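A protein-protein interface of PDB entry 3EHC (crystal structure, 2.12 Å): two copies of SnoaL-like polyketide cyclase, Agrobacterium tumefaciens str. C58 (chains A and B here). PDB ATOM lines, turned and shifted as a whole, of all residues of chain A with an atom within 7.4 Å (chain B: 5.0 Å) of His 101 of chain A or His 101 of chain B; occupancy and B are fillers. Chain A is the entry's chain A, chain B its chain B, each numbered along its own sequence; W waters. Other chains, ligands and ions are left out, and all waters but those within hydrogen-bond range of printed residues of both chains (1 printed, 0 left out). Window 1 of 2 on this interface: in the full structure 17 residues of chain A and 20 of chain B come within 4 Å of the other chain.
A ring nitrogen (ND1) of His 101 of chain A sits at hydrogen-bond distance from the backbone carbonyl oxygen of His 101 of chain B (2.8 Å).
The side-chain sulfur (SG) of Cys 99 of chain B is in hydrogen-bond range of the guanidinium group (NH2) of Arg 75 of chain B (3.4 Å). NH2 of Arg 75 of chain A lies within hydrogen-bond range of SG of Cys 99 of chain A. O of Val 102 of chain B sits at hydrogen-bond distance from N of Ala 74 of chain B, 2.9 Å away. The backbone NH of Phe 103 of chain A sits at hydrogen-bond distance from the backbone carbonyl oxygen of Trp 115 of chain A, 2.9 Å away. The backbone NH of Arg 75 of chain A sits at hydrogen-bond distance from the backbone carbonyl oxygen of Ile 64 of chain A (2.9 Å). N of His 101 of chain B lies within hydrogen-bond range of O of Val 117 of chain B.
CG2 of Ile 64 of chain A touches CD2 of Phe 103 of chain B, 3.97 Å away. CD1 of Ile 64 of chain A touches CE3 of Trp 115 of chain B, 3.6 Å away. C of Ala 73 of chain A touches CZ of Phe 103 of chain B, 3.8 Å away. Ala 74 of chain A touches Phe 103 of chain B. Arg 75 of chain A touches Trp 115 of chain B (CZ to CD1, 3.7 Å). Phe 103 of chain B touches His 101 of chain A. His 101 of chain A touches Trp 115 of chain B. Val 117 of chain B touches His 101 of chain A (CG2 to CE1, 3.6 Å). Trp 115 of chain A touches His 101 of chain B. Val 117 of chain B touches Val 117 of chain A.
Printed residues of chain B within 4 Å of His 101 of chain A: His 101, Phe 103, Trp 115, Ser 116 and Val 117. His 101 of chain B touches four residues of chain A. Of the printed residues of chain B, Phe 103 of chain A touches Ala 74 (3.3 Å), Arg 75 (3.4 Å) and His 101 (3.6 Å). Printed residues of chain B within 4 Å of Trp 115 of chain A: Arg 75 and His 101. Printed residues of chain B within 4 Å of Val 117 of chain A: His 101 and Val 117. The nearest printed residue of chain B that does not touch His 101 of chain A is Val 102 of chain B (4.3 Å).
Of the 10 printed residues of chain B, 7 touch a printed residue of chain A. Hydrophobic or aromatic side chains of chain B within 4 Å of the printed part of chain A: His 101, Phe 103, Trp 115 and Val 117. Hydrophobic or aromatic side chains of chain A that line the printed part of chain B: Ile 64, Ala 73, His 101, Phe 103, Trp 115 and Val 117. Among the printed residues, 20 pairs touch across the chains.
Ala 74 of chain A touches Phe 103 of chain B, and with the chains exchanged Phe 103 of chain A touches Ala 74 of chain B. Arg 75 of chain A touches Phe 103 of chain B, and with the chains exchanged Phe 103 of chain A touches Arg 75 of chain B. His 101 of chain A touches its own counterpart, His 101 of chain B. His 101 of chain A touches Phe 103 of chain B, and with the chains exchanged Phe 103 of chain A touches His 101 of chain B.
Water W1 bridges NH1 of Arg 75 of chain A (3.3 Å) and O of Ser 116 of chain B (3.5 Å).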
ATOM      1  N   ASN A  35      31.357  31.837   4.585  1.00  0.00           N
ATOM      2  CA  ASN A  35      30.591  31.915   5.821  1.00  0.00           C
ATOM      3  C   ASN A  35      30.986  33.090   6.709  1.00  0.00           C
ATOM      4  O   ASN A  35      31.161  32.934   7.905  1.00  0.00           O
ATOM      5  CB  ASN A  35      30.686  30.583   6.559  1.00  0.00           C
ATOM      6  CG  ASN A  35      29.845  29.493   5.900  1.00  0.00           C
ATOM      7  OD1 ASN A  35      29.118  29.722   4.922  1.00  0.00           O
ATOM      8  ND2 ASN A  35      29.958  28.301   6.421  1.00  0.00           N
ATOM      9  N   GLU A  63      23.963  17.359  -6.837  1.00  0.00           N
ATOM     10  CA  GLU A  63      22.659  16.789  -7.157  1.00  0.00           C
ATOM     11  C   GLU A  63      21.678  17.805  -7.703  1.00  0.00           C
ATOM     12  O   GLU A  63      20.795  17.458  -8.437  1.00  0.00           O
ATOM     13  CB  GLU A  63      22.027  16.181  -5.924  1.00  0.00           C
ATOM     14  CG  GLU A  63      22.645  14.845  -5.505  1.00  0.00           C
ATOM     15  CD  GLU A  63      21.769  14.126  -4.471  1.00  0.00           C
ATOM     16  OE1 GLU A  63      20.805  14.777  -3.950  1.00  0.00           O
ATOM     17  OE2 GLU A  63      22.052  12.916  -4.218  1.00  0.00           O
ATOM     18  N   ILE A  64      21.796  19.064  -7.307  1.00  0.00           N
ATOM     19  CA  ILE A  64      20.949  20.142  -7.853  1.00  0.00           C
ATOM     20  C   ILE A  64      21.809  21.372  -8.040  1.00  0.00           C
ATOM     21  O   ILE A  64      22.603  21.728  -7.163  1.00  0.00           O
ATOM     22  CB  ILE A  64      19.755  20.534  -6.911  1.00  0.00           C
ATOM     23  CG1 ILE A  64      19.042  19.284  -6.361  1.00  0.00           C
ATOM     24  CG2 ILE A  64      18.735  21.430  -7.651  1.00  0.00           C
ATOM     25  CD1 ILE A  64      17.918  19.588  -5.417  1.00  0.00           C
ATOM     26  N   ALA A  73      23.350  28.250  -6.617  1.00  0.00           N
ATOM     27  CA  ALA A  73      23.063  27.462  -5.401  1.00  0.00           C
ATOM     28  C   ALA A  73      23.222  25.984  -5.767  1.00  0.00           C
ATOM     29  O   ALA A  73      22.714  25.541  -6.803  1.00  0.00           O
ATOM     30  CB  ALA A  73      21.650  27.763  -4.886  1.00  0.00           C
ATOM     31  N   ALA A  74      23.946  25.238  -4.938  1.00  0.00           N
ATOM     32  CA  ALA A  74      24.211  23.836  -5.178  1.00  0.00           C
ATOM     33  C   ALA A  74      23.748  22.977  -4.006  1.00  0.00           C
ATOM     34  O   ALA A  74      23.976  23.311  -2.859  1.00  0.00           O
ATOM     35  CB  ALA A  74      25.714  23.608  -5.455  1.00  0.00           C
ATOM     36  N   ARG A  75      23.077  21.865  -4.308  1.00  0.00           N
ATOM     37  CA  ARG A  75      22.960  20.767  -3.332  1.00  0.00           C
ATOM     38  C   ARG A  75      23.989  19.732  -3.695  1.00  0.00           C
ATOM     39  O   ARG A  75      23.906  19.102  -4.747  1.00  0.00           O
ATOM     40  CB  ARG A  75      21.556  20.183  -3.332  1.00  0.00           C
ATOM     41  CG  ARG A  75      21.385  18.859  -2.545  1.00  0.00           C
ATOM     42  CD  ARG A  75      19.910  18.461  -2.496  1.00  0.00           C
ATOM     43  NE  ARG A  75      19.743  17.097  -2.003  1.00  0.00           N
ATOM     44  CZ  ARG A  75      19.531  16.756  -0.730  1.00  0.00           C
ATOM     45  NH1 ARG A  75      19.449  17.666   0.216  1.00  0.00           N
ATOM     46  NH2 ARG A  75      19.344  15.478  -0.400  1.00  0.00           N
ATOM     47  N   LEU A  76      24.967  19.569  -2.814  1.00  0.00           N
ATOM     48  CA  LEU A  76      26.072  18.634  -2.991  1.00  0.00           C
ATOM     49  C   LEU A  76      25.855  17.454  -2.067  1.00  0.00           C
ATOM     50  O   LEU A  76      25.514  17.638  -0.887  1.00  0.00           O
ATOM     51  CB  LEU A  76      27.370  19.317  -2.602  1.00  0.00           C
ATOM     52  CG  LEU A  76      27.800  20.511  -3.449  1.00  0.00           C
ATOM     53  CD1 LEU A  76      28.831  21.326  -2.696  1.00  0.00           C
ATOM     54  CD2 LEU A  76      28.372  19.985  -4.738  1.00  0.00           C
ATOM     55  N   PHE A  78      27.569  14.048  -0.351  1.00  0.00           N
ATOM     56  CA  PHE A  78      28.828  13.464   0.079  1.00  0.00           C
ATOM     57  C   PHE A  78      28.614  12.089   0.644  1.00  0.00           C
ATOM     58  O   PHE A  78      27.705  11.856   1.419  1.00  0.00           O
ATOM     59  CB  PHE A  78      29.487  14.330   1.136  1.00  0.00           C
ATOM     60  CG  PHE A  78      29.916  15.665   0.630  1.00  0.00           C
ATOM     61  CD1 PHE A  78      31.097  15.794  -0.093  1.00  0.00           C
ATOM     62  CD2 PHE A  78      29.122  16.807   0.845  1.00  0.00           C
ATOM     63  CE1 PHE A  78      31.517  17.059  -0.568  1.00  0.00           C
ATOM     64  CE2 PHE A  78      29.503  18.051   0.358  1.00  0.00           C
ATOM     65  CZ  PHE A  78      30.699  18.196  -0.332  1.00  0.00           C
ATOM     66  N   CYS A  99      24.519  15.912   2.926  1.00  0.00           N
ATOM     67  CA  CYS A  99      24.535  16.962   1.940  1.00  0.00           C
ATOM     68  C   CYS A  99      24.982  18.262   2.531  1.00  0.00           C
ATOM     69  O   CYS A  99      24.936  18.457   3.737  1.00  0.00           O
ATOM     70  CB  CYS A  99      23.132  17.151   1.350  1.00  0.00           C
ATOM     71  SG  CYS A  99      22.660  15.691   0.417  1.00  0.00           S
ATOM     72  N   GLU A 100      25.398  19.124   1.620  1.00  0.00           N
ATOM     73  CA  GLU A 100      25.712  20.513   1.865  1.00  0.00           C
ATOM     74  C   GLU A 100      24.831  21.344   0.920  1.00  0.00           C
ATOM     75  O   GLU A 100      24.681  20.995  -0.262  1.00  0.00           O
ATOM     76  CB  GLU A 100      27.184  20.761   1.533  1.00  0.00           C
ATOM     77  CG  GLU A 100      27.598  22.227   1.572  1.00  0.00           C
ATOM     78  CD  GLU A 100      29.064  22.477   1.155  1.00  0.00           C
ATOM     79  OE1 GLU A 100      29.823  21.496   0.918  1.00  0.00           O
ATOM     80  OE2 GLU A 100      29.457  23.678   1.080  1.00  0.00           O
ATOM     81  N   HIS A 101      24.226  22.402   1.440  1.00  0.00           N
ATOM     82  CA  HIS A 101      23.470  23.354   0.612  1.00  0.00           C
ATOM     83  C   HIS A 101      24.257  24.674   0.658  1.00  0.00           C
ATOM     84  O   HIS A 101      24.490  25.207   1.735  1.00  0.00           O
ATOM     85  CB  HIS A 101      22.035  23.539   1.157  1.00  0.00           C
ATOM     86  CG  HIS A 101      21.109  22.380   0.896  1.00  0.00           C
ATOM     87  ND1 HIS A 101      19.762  22.423   1.196  1.00  0.00           N
ATOM     88  CD2 HIS A 101      21.333  21.152   0.372  1.00  0.00           C
ATOM     89  CE1 HIS A 101      19.204  21.269   0.876  1.00  0.00           C
ATOM     90  NE2 HIS A 101      20.128  20.488   0.349  1.00  0.00           N
ATOM     91  N   VAL A 102      24.709  25.153  -0.509  1.00  0.00           N
ATOM     92  CA  VAL A 102      25.667  26.270  -0.570  1.00  0.00           C
ATOM     93  C   VAL A 102      25.252  27.290  -1.656  1.00  0.00           C
ATOM     94  O   VAL A 102      24.796  26.914  -2.714  1.00  0.00           O
ATOM     95  CB  VAL A 102      27.135  25.749  -0.742  1.00  0.00           C
ATOM     96  CG1 VAL A 102      27.229  24.811  -1.863  1.00  0.00           C
ATOM     97  CG2 VAL A 102      28.210  26.958  -0.873  1.00  0.00           C
ATOM     98  N   PHE A 103      25.352  28.578  -1.317  1.00  0.00           N
ATOM     99  CA  PHE A 103      25.098  29.702  -2.215  1.00  0.00           C
ATOM    100  C   PHE A 103      26.427  30.382  -2.537  1.00  0.00           C
ATOM    101  O   PHE A 103      27.262  30.595  -1.662  1.00  0.00           O
ATOM    102  CB  PHE A 103      24.143  30.714  -1.563  1.00  0.00           C
ATOM    103  CG  PHE A 103      22.729  30.237  -1.447  1.00  0.00           C
ATOM    104  CD1 PHE A 103      22.358  29.357  -0.435  1.00  0.00           C
ATOM    105  CD2 PHE A 103      21.753  30.660  -2.359  1.00  0.00           C
ATOM    106  CE1 PHE A 103      21.036  28.886  -0.325  1.00  0.00           C
ATOM    107  CE2 PHE A 103      20.435  30.194  -2.254  1.00  0.00           C
ATOM    108  CZ  PHE A 103      20.089  29.295  -1.229  1.00  0.00           C
ATOM    109  N   TYR A 104      26.616  30.720  -3.809  1.00  0.00           N
ATOM    110  CA  TYR A 104      27.820  31.419  -4.266  1.00  0.00           C
ATOM    111  C   TYR A 104      27.424  32.737  -4.911  1.00  0.00           C
ATOM    112  O   TYR A 104      26.502  32.777  -5.704  1.00  0.00           O
ATOM    113  CB  TYR A 104      28.578  30.551  -5.301  1.00  0.00           C
ATOM    114  CG  TYR A 104      29.009  29.200  -4.799  1.00  0.00           C
ATOM    115  CD1 TYR A 104      28.157  28.129  -4.875  1.00  0.00           C
ATOM    116  CD2 TYR A 104      30.277  29.004  -4.248  1.00  0.00           C
ATOM    117  CE1 TYR A 104      28.530  26.904  -4.410  1.00  0.00           C
ATOM    118  CE2 TYR A 104      30.669  27.771  -3.785  1.00  0.00           C
ATOM    119  CZ  TYR A 104      29.778  26.719  -3.868  1.00  0.00           C
ATOM    120  OH  TYR A 104      30.104  25.456  -3.444  1.00  0.00           O
ATOM    121  N   VAL A 114      30.595  33.007  -0.235  1.00  0.00           N
ATOM    122  CA  VAL A 114      30.027  31.663  -0.096  1.00  0.00           C
ATOM    123  C   VAL A 114      29.241  31.611   1.219  1.00  0.00           C
ATOM    124  O   VAL A 114      29.708  32.111   2.230  1.00  0.00           O
ATOM    125  CB  VAL A 114      31.125  30.578  -0.129  1.00  0.00           C
ATOM    126  CG1 VAL A 114      30.514  29.164  -0.080  1.00  0.00           C
ATOM    127  CG2 VAL A 114      32.033  30.732  -1.382  1.00  0.00           C
ATOM    128  N   TRP A 115      28.022  31.054   1.161  1.00  0.00           N
ATOM    129  CA  TRP A 115      27.285  30.685   2.342  1.00  0.00           C
ATOM    130  C   TRP A 115      26.946  29.217   2.284  1.00  0.00           C
ATOM    131  O   TRP A 115      26.229  28.800   1.415  1.00  0.00           O
ATOM    132  CB  TRP A 115      25.996  31.477   2.489  1.00  0.00           C
ATOM    133  CG  TRP A 115      26.223  32.918   2.572  1.00  0.00           C
ATOM    134  CD1 TRP A 115      26.318  33.674   3.706  1.00  0.00           C
ATOM    135  CD2 TRP A 115      26.403  33.806   1.462  1.00  0.00           C
ATOM    136  NE1 TRP A 115      26.558  34.982   3.360  1.00  0.00           N
ATOM    137  CE2 TRP A 115      26.608  35.094   1.991  1.00  0.00           C
ATOM    138  CE3 TRP A 115      26.423  33.628   0.055  1.00  0.00           C
ATOM    139  CZ2 TRP A 115      26.824  36.226   1.167  1.00  0.00           C
ATOM    140  CZ3 TRP A 115      26.626  34.747  -0.770  1.00  0.00           C
ATOM    141  CH2 TRP A 115      26.806  36.038  -0.205  1.00  0.00           C
ATOM    142  N   SER A 116      27.467  28.440   3.243  1.00  0.00           N
ATOM    143  CA  SER A 116      27.337  26.983   3.260  1.00  0.00           C
ATOM    144  C   SER A 116      26.717  26.472   4.527  1.00  0.00           C
ATOM    145  O   SER A 116      27.082  26.932   5.575  1.00  0.00           O
ATOM    146  CB  SER A 116      28.723  26.349   3.196  1.00  0.00           C
ATOM    147  OG  SER A 116      28.582  24.958   3.389  1.00  0.00           O
ATOM    148  N   VAL A 117      25.771  25.529   4.413  1.00  0.00           N
ATOM    149  CA  VAL A 117      25.219  24.803   5.566  1.00  0.00           C
ATOM    150  C   VAL A 117      25.341  23.296   5.269  1.00  0.00           C
ATOM    151  O   VAL A 117      24.985  22.859   4.174  1.00  0.00           O
ATOM    152  CB  VAL A 117      23.765  25.207   5.928  1.00  0.00           C
ATOM    153  CG1 VAL A 117      23.306  24.471   7.120  1.00  0.00           C
ATOM    154  CG2 VAL A 117      23.678  26.658   6.297  1.00  0.00           C
ATOM    155  N   LEU A 118      25.914  22.535   6.211  1.00  0.00           N
ATOM    156  CA  LEU A 118      26.010  21.072   6.116  1.00  0.00           C
ATOM    157  C   LEU A 118      24.984  20.413   7.024  1.00  0.00           C
ATOM    158  O   LEU A 118      24.605  20.932   8.066  1.00  0.00           O
ATOM    159  CB  LEU A 118      27.401  20.511   6.441  1.00  0.00           C
ATOM    160  CG  LEU A 118      28.730  21.024   5.839  1.00  0.00           C
ATOM    161  CD1 LEU A 118      29.832  20.032   6.239  1.00  0.00           C
ATOM    162  CD2 LEU A 118      28.764  21.251   4.312  1.00  0.00           C
ATOM    163  N   ASP A 119      24.529  19.238   6.599  1.00  0.00           N
ATOM    164  CA  ASP A 119      23.489  18.491   7.304  1.00  0.00           C
ATOM    165  C   ASP A 119      24.095  17.642   8.460  1.00  0.00           C
ATOM    166  O   ASP A 119      24.328  16.431   8.331  1.00  0.00           O
ATOM    167  CB  ASP A 119      22.754  17.604   6.293  1.00  0.00           C
ATOM    168  CG  ASP A 119      21.438  17.043   6.819  1.00  0.00           C
ATOM    169  OD1 ASP A 119      21.126  17.227   7.998  1.00  0.00           O
ATOM    170  OD2 ASP A 119      20.705  16.405   6.027  1.00  0.00           O
ATOM    171  N   ALA B  74      16.508  29.121  -1.654  1.00  0.00           N
ATOM    172  CA  ALA B  74      16.415  30.243  -0.700  1.00  0.00           C
ATOM    173  C   ALA B  74      17.387  30.071   0.470  1.00  0.00           C
ATOM    174  O   ALA B  74      17.518  28.976   1.009  1.00  0.00           O
ATOM    175  CB  ALA B  74      14.971  30.383  -0.175  1.00  0.00           C
ATOM    176  N   ARG B  75      18.096  31.146   0.825  1.00  0.00           N
ATOM    177  CA  ARG B  75      18.713  31.275   2.137  1.00  0.00           C
ATOM    178  C   ARG B  75      17.768  32.124   2.981  1.00  0.00           C
ATOM    179  O   ARG B  75      17.592  33.296   2.714  1.00  0.00           O
ATOM    180  CB  ARG B  75      20.088  31.920   2.057  1.00  0.00           C
ATOM    181  CG  ARG B  75      20.725  32.188   3.399  1.00  0.00           C
ATOM    182  CD  ARG B  75      22.096  32.831   3.126  1.00  0.00           C
ATOM    183  NE  ARG B  75      22.675  33.474   4.288  1.00  0.00           N
ATOM    184  CZ  ARG B  75      23.319  32.811   5.244  1.00  0.00           C
ATOM    185  NH1 ARG B  75      23.500  31.486   5.184  1.00  0.00           N
ATOM    186  NH2 ARG B  75      23.823  33.480   6.235  1.00  0.00           N
ATOM    187  N   CYS B  99      20.239  30.038  10.021  1.00  0.00           N
ATOM    188  CA  CYS B  99      19.720  30.039   8.663  1.00  0.00           C
ATOM    189  C   CYS B  99      19.255  28.657   8.247  1.00  0.00           C
ATOM    190  O   CYS B  99      19.628  27.648   8.845  1.00  0.00           O
ATOM    191  CB  CYS B  99      20.770  30.547   7.688  1.00  0.00           C
ATOM    192  SG  CYS B  99      21.104  32.272   7.850  1.00  0.00           S
ATOM    193  N   GLU B 100      18.418  28.651   7.219  1.00  0.00           N
ATOM    194  CA  GLU B 100      17.969  27.443   6.544  1.00  0.00           C
ATOM    195  C   GLU B 100      18.261  27.641   5.048  1.00  0.00           C
ATOM    196  O   GLU B 100      17.965  28.703   4.491  1.00  0.00           O
ATOM    197  CB  GLU B 100      16.475  27.244   6.738  1.00  0.00           C
ATOM    198  CG  GLU B 100      15.935  25.924   6.171  1.00  0.00           C
ATOM    199  CD  GLU B 100      14.401  25.868   6.137  1.00  0.00           C
ATOM    200  OE1 GLU B 100      13.742  26.723   6.765  1.00  0.00           O
ATOM    201  OE2 GLU B 100      13.848  24.954   5.481  1.00  0.00           O
ATOM    202  N   HIS B 101      18.863  26.627   4.427  1.00  0.00           N
ATOM    203  CA  HIS B 101      19.093  26.599   2.983  1.00  0.00           C
ATOM    204  C   HIS B 101      18.207  25.536   2.363  1.00  0.00           C
ATOM    205  O   HIS B 101      18.309  24.354   2.666  1.00  0.00           O
ATOM    206  CB  HIS B 101      20.529  26.287   2.665  1.00  0.00           C
ATOM    207  CG  HIS B 101      21.468  27.402   3.004  1.00  0.00           C
ATOM    208  ND1 HIS B 101      22.788  27.405   2.619  1.00  0.00           N
ATOM    209  CD2 HIS B 101      21.274  28.545   3.700  1.00  0.00           C
ATOM    210  CE1 HIS B 101      23.366  28.511   3.045  1.00  0.00           C
ATOM    211  NE2 HIS B 101      22.467  29.220   3.702  1.00  0.00           N
ATOM    212  N   VAL B 102      17.347  25.964   1.458  1.00  0.00           N
ATOM    213  CA  VAL B 102      16.283  25.098   0.983  1.00  0.00           C
ATOM    214  C   VAL B 102      16.117  25.217  -0.538  1.00  0.00           C
ATOM    215  O   VAL B 102      16.185  26.296  -1.104  1.00  0.00           O
ATOM    216  CB  VAL B 102      14.960  25.369   1.799  1.00  0.00           C
ATOM    217  CG1 VAL B 102      14.654  26.829   1.801  1.00  0.00           C
ATOM    218  CG2 VAL B 102      13.751  24.468   1.327  1.00  0.00           C
ATOM    219  N   PHE B 103      15.966  24.060  -1.171  1.00  0.00           N
ATOM    220  CA  PHE B 103      15.660  23.922  -2.605  1.00  0.00           C
ATOM    221  C   PHE B 103      14.197  23.498  -2.807  1.00  0.00           C
ATOM    222  O   PHE B 103      13.690  22.631  -2.089  1.00  0.00           O
ATOM    223  CB  PHE B 103      16.582  22.868  -3.267  1.00  0.00           C
ATOM    224  CG  PHE B 103      17.988  23.316  -3.407  1.00  0.00           C
ATOM    225  CD1 PHE B 103      18.875  23.192  -2.340  1.00  0.00           C
ATOM    226  CD2 PHE B 103      18.442  23.921  -4.579  1.00  0.00           C
ATOM    227  CE1 PHE B 103      20.167  23.661  -2.443  1.00  0.00           C
ATOM    228  CE2 PHE B 103      19.780  24.378  -4.668  1.00  0.00           C
ATOM    229  CZ  PHE B 103      20.605  24.247  -3.615  1.00  0.00           C
ATOM    230  N   TRP B 115      13.913  20.255  -0.426  1.00  0.00           N
ATOM    231  CA  TRP B 115      15.087  19.734   0.274  1.00  0.00           C
ATOM    232  C   TRP B 115      15.629  20.849   1.139  1.00  0.00           C
ATOM    233  O   TRP B 115      16.085  21.857   0.617  1.00  0.00           O
ATOM    234  CB  TRP B 115      16.156  19.240  -0.730  1.00  0.00           C
ATOM    235  CG  TRP B 115      15.726  18.067  -1.575  1.00  0.00           C
ATOM    236  CD1 TRP B 115      15.861  16.746  -1.257  1.00  0.00           C
ATOM    237  CD2 TRP B 115      15.118  18.110  -2.877  1.00  0.00           C
ATOM    238  NE1 TRP B 115      15.378  15.968  -2.278  1.00  0.00           N
ATOM    239  CE2 TRP B 115      14.918  16.775  -3.286  1.00  0.00           C
ATOM    240  CE3 TRP B 115      14.712  19.151  -3.742  1.00  0.00           C
ATOM    241  CZ2 TRP B 115      14.323  16.440  -4.536  1.00  0.00           C
ATOM    242  CZ3 TRP B 115      14.124  18.818  -4.993  1.00  0.00           C
ATOM    243  CH2 TRP B 115      13.945  17.470  -5.371  1.00  0.00           C
ATOM    244  N   SER B 116      15.587  20.654   2.456  1.00  0.00           N
ATOM    245  CA  SER B 116      15.952  21.691   3.403  1.00  0.00           C
ATOM    246  C   SER B 116      17.047  21.217   4.360  1.00  0.00           C
ATOM    247  O   SER B 116      17.046  20.072   4.802  1.00  0.00           O
ATOM    248  CB  SER B 116      14.708  22.122   4.175  1.00  0.00           C
ATOM    249  OG  SER B 116      15.083  22.743   5.383  1.00  0.00           O
ATOM    250  N   VAL B 117      17.992  22.109   4.650  1.00  0.00           N
ATOM    251  CA  VAL B 117      19.016  21.901   5.680  1.00  0.00           C
ATOM    252  C   VAL B 117      19.028  23.138   6.586  1.00  0.00           C
ATOM    253  O   VAL B 117      19.130  24.261   6.098  1.00  0.00           O
ATOM    254  CB  VAL B 117      20.436  21.609   5.044  1.00  0.00           C
ATOM    255  CG1 VAL B 117      21.436  21.429   6.093  1.00  0.00           C
ATOM    256  CG2 VAL B 117      20.405  20.365   4.157  1.00  0.00           C
HETATM  257  O   HOH W   1      18.532  17.257   3.361  1.00  0.00           O
